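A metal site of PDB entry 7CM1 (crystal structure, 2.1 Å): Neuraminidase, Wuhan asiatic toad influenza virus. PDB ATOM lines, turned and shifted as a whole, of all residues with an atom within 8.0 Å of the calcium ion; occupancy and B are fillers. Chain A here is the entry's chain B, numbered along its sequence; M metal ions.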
ATOM      1  N   MET A 194      29.588  -9.227  20.203  1.00  0.00           N
ATOM      2  CA  MET A 194      28.649  -9.222  19.084  1.00  0.00           C
ATOM      3  C   MET A 194      29.467  -9.225  17.799  1.00  0.00           C
ATOM      4  O   MET A 194      30.065  -8.204  17.427  1.00  0.00           O
ATOM      5  CB  MET A 194      27.691  -8.026  19.171  1.00  0.00           C
ATOM      6  CG  MET A 194      27.272  -7.380  17.847  1.00  0.00           C
ATOM      7  SD  MET A 194      26.269  -8.398  16.761  1.00  0.00           S
ATOM      8  CE  MET A 194      24.684  -8.271  17.593  1.00  0.00           C
ATOM      9  N   ARG A 213      31.171  -7.515  11.383  1.00  0.00           N
ATOM     10  CA  ARG A 213      30.222  -6.436  11.653  1.00  0.00           C
ATOM     11  C   ARG A 213      29.795  -6.522  13.110  1.00  0.00           C
ATOM     12  O   ARG A 213      29.496  -7.609  13.610  1.00  0.00           O
ATOM     13  CB  ARG A 213      29.006  -6.582  10.745  1.00  0.00           C
ATOM     14  CG  ARG A 213      27.751  -5.872  11.218  1.00  0.00           C
ATOM     15  CD  ARG A 213      26.679  -6.100  10.201  1.00  0.00           C
ATOM     16  NE  ARG A 213      25.474  -5.327  10.420  1.00  0.00           N
ATOM     17  CZ  ARG A 213      24.493  -5.266   9.526  1.00  0.00           C
ATOM     18  NH1 ARG A 213      24.584  -5.941   8.388  1.00  0.00           N
ATOM     19  NH2 ARG A 213      23.409  -4.545   9.773  1.00  0.00           N
ATOM     20  N   ASP A 214      29.791  -5.383  13.783  1.00  0.00           N
ATOM     21  CA  ASP A 214      29.243  -5.267  15.134  1.00  0.00           C
ATOM     22  C   ASP A 214      27.979  -4.428  14.979  1.00  0.00           C
ATOM     23  O   ASP A 214      28.051  -3.233  14.677  1.00  0.00           O
ATOM     24  CB  ASP A 214      30.248  -4.631  16.085  1.00  0.00           C
ATOM     25  CG  ASP A 214      29.807  -4.649  17.557  1.00  0.00           C
ATOM     26  OD1 ASP A 214      28.666  -4.254  17.845  1.00  0.00           O
ATOM     27  OD2 ASP A 214      30.608  -5.058  18.429  1.00  0.00           O
ATOM     28  N   ASN A 215      26.823  -5.055  15.162  1.00  0.00           N
ATOM     29  CA  ASN A 215      25.598  -4.320  14.887  1.00  0.00           C
ATOM     30  C   ASN A 215      25.191  -3.410  16.031  1.00  0.00           C
ATOM     31  O   ASN A 215      24.184  -2.692  15.916  1.00  0.00           O
ATOM     32  CB  ASN A 215      24.463  -5.267  14.540  1.00  0.00           C
ATOM     33  CG  ASN A 215      23.499  -4.663  13.555  1.00  0.00           C
ATOM     34  OD1 ASN A 215      23.917  -4.078  12.544  1.00  0.00           O
ATOM     35  ND2 ASN A 215      22.203  -4.759  13.854  1.00  0.00           N
ATOM     36  N   THR A 216      25.936  -3.421  17.128  1.00  0.00           N
ATOM     37  CA  THR A 216      25.726  -2.511  18.234  1.00  0.00           C
ATOM     38  C   THR A 216      26.257  -1.121  17.848  1.00  0.00           C
ATOM     39  O   THR A 216      26.751  -0.915  16.741  1.00  0.00           O
ATOM     40  CB  THR A 216      26.364  -3.105  19.486  1.00  0.00           C
ATOM     41  OG1 THR A 216      25.395  -3.159  20.544  1.00  0.00           O
ATOM     42  CG2 THR A 216      27.621  -2.372  19.952  1.00  0.00           C
ATOM     43  N   ALA A 217      26.122  -0.150  18.772  1.00  0.00           N
ATOM     44  CA  ALA A 217      26.617   1.206  18.540  1.00  0.00           C
ATOM     45  C   ALA A 217      28.090   1.247  18.135  1.00  0.00           C
ATOM     46  O   ALA A 217      28.529   2.235  17.551  1.00  0.00           O
ATOM     47  CB  ALA A 217      26.402   2.042  19.798  1.00  0.00           C
ATOM     48  N   ASN A 218      28.851   0.204  18.451  1.00  0.00           N
ATOM     49  CA  ASN A 218      30.267   0.156  18.132  1.00  0.00           C
ATOM     50  C   ASN A 218      30.509   0.290  16.629  1.00  0.00           C
ATOM     51  O   ASN A 218      29.857  -0.374  15.815  1.00  0.00           O
ATOM     52  CB  ASN A 218      30.841  -1.168  18.646  1.00  0.00           C
ATOM     53  CG  ASN A 218      32.299  -1.344  18.325  1.00  0.00           C
ATOM     54  OD1 ASN A 218      33.036  -0.371  18.145  1.00  0.00           O
ATOM     55  ND2 ASN A 218      32.746  -2.596  18.281  1.00  0.00           N
ATOM     56  N   SER A 219      31.458   1.155  16.261  1.00  0.00           N
ATOM     57  CA  SER A 219      31.881   1.331  14.875  1.00  0.00           C
ATOM     58  C   SER A 219      33.219   0.677  14.571  1.00  0.00           C
ATOM     59  O   SER A 219      33.625   0.661  13.407  1.00  0.00           O
ATOM     60  CB  SER A 219      31.956   2.814  14.525  1.00  0.00           C
ATOM     61  OG  SER A 219      30.670   3.385  14.487  1.00  0.00           O
ATOM     62  N   ARG A 220      33.918   0.163  15.575  1.00  0.00           N
ATOM     63  CA  ARG A 220      35.171  -0.536  15.336  1.00  0.00           C
ATOM     64  C   ARG A 220      34.868  -1.999  15.021  1.00  0.00           C
ATOM     65  O   ARG A 220      34.250  -2.699  15.831  1.00  0.00           O
ATOM     66  CB  ARG A 220      36.094  -0.395  16.554  1.00  0.00           C
ATOM     67  CG  ARG A 220      36.168   1.049  17.027  1.00  0.00           C
ATOM     68  CD  ARG A 220      37.551   1.496  17.454  1.00  0.00           C
ATOM     69  NE  ARG A 220      37.877   1.077  18.799  1.00  0.00           N
ATOM     70  CZ  ARG A 220      38.828   1.639  19.555  1.00  0.00           C
ATOM     71  NH1 ARG A 220      39.556   2.664  19.105  1.00  0.00           N
ATOM     72  NH2 ARG A 220      39.044   1.170  20.771  1.00  0.00           N
ATOM     73  N   ARG A 221      35.298  -2.460  13.850  1.00  0.00           N
ATOM     74  CA  ARG A 221      34.992  -3.815  13.437  1.00  0.00           C
ATOM     75  C   ARG A 221      35.720  -4.824  14.312  1.00  0.00           C
ATOM     76  O   ARG A 221      36.904  -4.656  14.618  1.00  0.00           O
ATOM     77  CB  ARG A 221      35.381  -4.040  11.984  1.00  0.00           C
ATOM     78  CG  ARG A 221      34.468  -3.368  11.012  1.00  0.00           C
ATOM     79  CD  ARG A 221      34.829  -3.721   9.591  1.00  0.00           C
ATOM     80  NE  ARG A 221      33.966  -3.048   8.627  1.00  0.00           N
ATOM     81  CZ  ARG A 221      32.666  -3.297   8.499  1.00  0.00           C
ATOM     82  NH1 ARG A 221      32.067  -4.210   9.266  1.00  0.00           N
ATOM     83  NH2 ARG A 221      31.951  -2.640   7.585  1.00  0.00           N
ATOM     84  N   PRO A 222      35.036  -5.877  14.745  1.00  0.00           N
ATOM     85  CA  PRO A 222      35.751  -7.010  15.321  1.00  0.00           C
ATOM     86  C   PRO A 222      36.622  -7.670  14.264  1.00  0.00           C
ATOM     87  O   PRO A 222      36.228  -7.793  13.104  1.00  0.00           O
ATOM     88  CB  PRO A 222      34.630  -7.944  15.794  1.00  0.00           C
ATOM     89  CG  PRO A 222      33.382  -7.062  15.844  1.00  0.00           C
ATOM     90  CD  PRO A 222      33.575  -6.055  14.781  1.00  0.00           C
ATOM     91  N   ASP A 245      33.127   0.774   9.929  1.00  0.00           N
ATOM     92  CA  ASP A 245      31.733   0.368   9.863  1.00  0.00           C
ATOM     93  C   ASP A 245      30.844   1.531   9.410  1.00  0.00           C
ATOM     94  O   ASP A 245      31.300   2.669   9.232  1.00  0.00           O
ATOM     95  CB  ASP A 245      31.290  -0.180  11.227  1.00  0.00           C
ATOM     96  CG  ASP A 245      30.043  -1.058  11.135  1.00  0.00           C
ATOM     97  OD1 ASP A 245      29.562  -1.352  10.009  1.00  0.00           O
ATOM     98  OD2 ASP A 245      29.528  -1.427  12.211  1.00  0.00           O
ATOM     99  N   CYS A 246      29.553   1.233   9.222  1.00  0.00           N
ATOM    100  CA  CYS A 246      28.506   2.147   8.783  1.00  0.00           C
ATOM    101  C   CYS A 246      27.215   1.760   9.490  1.00  0.00           C
ATOM    102  O   CYS A 246      26.754   0.617   9.341  1.00  0.00           O
ATOM    103  CB  CYS A 246      28.358   2.104   7.255  1.00  0.00           C
ATOM    104  SG  CYS A 246      27.053   3.160   6.555  1.00  0.00           S
ATOM    105  N   PRO A 247      26.602   2.665  10.283  1.00  0.00           N
ATOM    106  CA  PRO A 247      27.013   4.050  10.490  1.00  0.00           C
ATOM    107  C   PRO A 247      28.170   4.199  11.471  1.00  0.00           C
ATOM    108  O   PRO A 247      28.546   3.241  12.151  1.00  0.00           O
ATOM    109  CB  PRO A 247      25.751   4.690  11.072  1.00  0.00           C
ATOM    110  CG  PRO A 247      25.192   3.625  11.885  1.00  0.00           C
ATOM    111  CD  PRO A 247      25.426   2.337  11.117  1.00  0.00           C
ATOM    112  N   ARG A 248      28.690   5.419  11.548  1.00  0.00           N
ATOM    113  CA  ARG A 248      29.879   5.687  12.335  1.00  0.00           C
ATOM    114  C   ARG A 248      29.993   7.193  12.524  1.00  0.00           C
ATOM    115  O   ARG A 248      29.423   7.965  11.741  1.00  0.00           O
ATOM    116  CB  ARG A 248      31.131   5.142  11.637  1.00  0.00           C
ATOM    117  CG  ARG A 248      31.436   5.815  10.311  1.00  0.00           C
ATOM    118  CD  ARG A 248      32.809   5.444   9.793  1.00  0.00           C
ATOM    119  NE  ARG A 248      32.786   5.345   8.336  1.00  0.00           N
ATOM    120  CZ  ARG A 248      33.206   6.297   7.514  1.00  0.00           C
ATOM    121  NH1 ARG A 248      33.713   7.417   8.008  1.00  0.00           N
ATOM    122  NH2 ARG A 248      33.120   6.129   6.199  1.00  0.00           N
ATOM    123  N   PHE A 260      33.989   1.623  20.285  1.00  0.00           N
ATOM    124  CA  PHE A 260      33.807   3.048  20.061  1.00  0.00           C
ATOM    125  C   PHE A 260      32.741   3.296  19.012  1.00  0.00           C
ATOM    126  O   PHE A 260      32.766   2.678  17.935  1.00  0.00           O
ATOM    127  CB  PHE A 260      35.105   3.742  19.629  1.00  0.00           C
ATOM    128  CG  PHE A 260      34.949   5.230  19.472  1.00  0.00           C
ATOM    129  CD1 PHE A 260      34.693   5.791  18.234  1.00  0.00           C
ATOM    130  CD2 PHE A 260      35.017   6.069  20.574  1.00  0.00           C
ATOM    131  CE1 PHE A 260      34.516   7.159  18.107  1.00  0.00           C
ATOM    132  CE2 PHE A 260      34.854   7.441  20.455  1.00  0.00           C
ATOM    133  CZ  PHE A 260      34.606   7.996  19.219  1.00  0.00           C
ATOM    134  N   GLY A 261      31.832   4.201  19.301  1.00  0.00           N
ATOM    135  CA  GLY A 261      30.753   4.526  18.398  1.00  0.00           C
ATOM    136  C   GLY A 261      29.491   4.919  19.143  1.00  0.00           C
ATOM    137  O   GLY A 261      29.252   4.540  20.283  1.00  0.00           O
ATOM    138  N   SER A 262      28.642   5.697  18.462  1.00  0.00           N
ATOM    139  CA  SER A 262      27.402   6.201  19.046  1.00  0.00           C
ATOM    140  C   SER A 262      26.162   5.846  18.220  1.00  0.00           C
ATOM    141  O   SER A 262      25.038   6.159  18.650  1.00  0.00           O
ATOM    142  CB  SER A 262      27.497   7.726  19.199  1.00  0.00           C
ATOM    143  OG  SER A 262      28.159   8.290  18.071  1.00  0.00           O
ATOM    144  N   LEU A 263      26.320   5.205  17.072  1.00  0.00           N
ATOM    145  CA  LEU A 263      25.239   4.981  16.137  1.00  0.00           C
ATOM    146  C   LEU A 263      25.040   3.480  15.951  1.00  0.00           C
ATOM    147  O   LEU A 263      25.852   2.807  15.300  1.00  0.00           O
ATOM    148  CB  LEU A 263      25.518   5.685  14.804  1.00  0.00           C
ATOM    149  CG  LEU A 263      25.844   7.179  14.957  1.00  0.00           C
ATOM    150  CD1 LEU A 263      27.354   7.408  15.113  1.00  0.00           C
ATOM    151  CD2 LEU A 263      25.274   8.010  13.810  1.00  0.00           C
ATOM    152  N   ALA A 264      23.962   2.949  16.531  1.00  0.00           N
ATOM    153  CA  ALA A 264      23.648   1.533  16.359  1.00  0.00           C
ATOM    154  C   ALA A 264      23.496   1.215  14.876  1.00  0.00           C
ATOM    155  O   ALA A 264      23.213   2.083  14.050  1.00  0.00           O
ATOM    156  CB  ALA A 264      22.388   1.163  17.123  1.00  0.00           C
ATOM    157  N   GLY A 265      23.690  -0.042  14.534  1.00  0.00           N
ATOM    158  CA  GLY A 265      23.677  -0.472  13.156  1.00  0.00           C
ATOM    159  C   GLY A 265      25.004  -1.076  12.758  1.00  0.00           C
ATOM    160  O   GLY A 265      25.843  -1.394  13.596  1.00  0.00           O
ATOM    161  N   GLY A 266      25.190  -1.253  11.456  1.00  0.00           N
ATOM    162  CA  GLY A 266      26.373  -1.952  11.004  1.00  0.00           C
ATOM    163  C   GLY A 266      26.258  -2.333   9.545  1.00  0.00           C
ATOM    164  O   GLY A 266      25.197  -2.225   8.921  1.00  0.00           O
ATOM    165  N   LEU A 267      27.390  -2.786   9.015  1.00  0.00           N
ATOM    166  CA  LEU A 267      27.467  -3.140   7.605  1.00  0.00           C
ATOM    167  C   LEU A 267      28.609  -4.120   7.408  1.00  0.00           C
ATOM    168  O   LEU A 267      29.683  -3.957   7.997  1.00  0.00           O
ATOM    169  CB  LEU A 267      27.663  -1.895   6.742  1.00  0.00           C
ATOM    170  CG  LEU A 267      27.796  -2.160   5.247  1.00  0.00           C
ATOM    171  CD1 LEU A 267      26.456  -2.628   4.679  1.00  0.00           C
ATOM    172  CD2 LEU A 267      28.285  -0.881   4.570  1.00  0.00           C
HETATM  173 CA    CA M   1      27.888  -0.824  14.432  1.00  0.00          CA
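O of Asp 245 sits at hydrogen-bond distance from NE of Arg 248 (3.2 Å). N of Gly 266 sits close to O of Cys 246, at 3.2 Å. OD1 of Asp 245 is in hydrogen-bond range of N of Leu 267 (2.8 Å). The side-chain amide oxygen (OD1) of Asn 218 sits close to the backbone carbonyl oxygen (O) of Phe 260 (3.1 Å). O of Gly 266 sits at hydrogen-bond distance from NH2 of Arg 213 (3.1 Å). N of Thr 216 sits at hydrogen-bond distance from OD1 of Asp 214. The side-chain amide nitrogen (ND2) of Asn 218 is in hydrogen-bond range of the side-chain carboxylate (OD2) of Asp 214, 3.3 Å away. The backbone NH of Gly 266 lies within hydrogen-bond range of the side-chain amide oxygen of Asn 215.
CA of Gly 266 touches the calcium ion, at 3.9 Å. Six residues have an atom within 4 Å of the calcium ion: Asp 214, Thr 216, Asn 218, Asp 245, Gly 265 and Gly 266. The nearest printed residue that does not touch the calcium ion is Asn 215 (4.1 Å).
The backbone carbonyl oxygen (O) of Gly 265 binds the calcium ion, at 2.3 Å. O of Asp 214 binds the calcium ion, 2.4 Å away. O of Asn 218 is bound to the calcium ion (2.4 Å). O of Thr 216 is bound to the calcium ion. OD2 of Asp 245 is bound to the calcium ion (2.8 Å).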
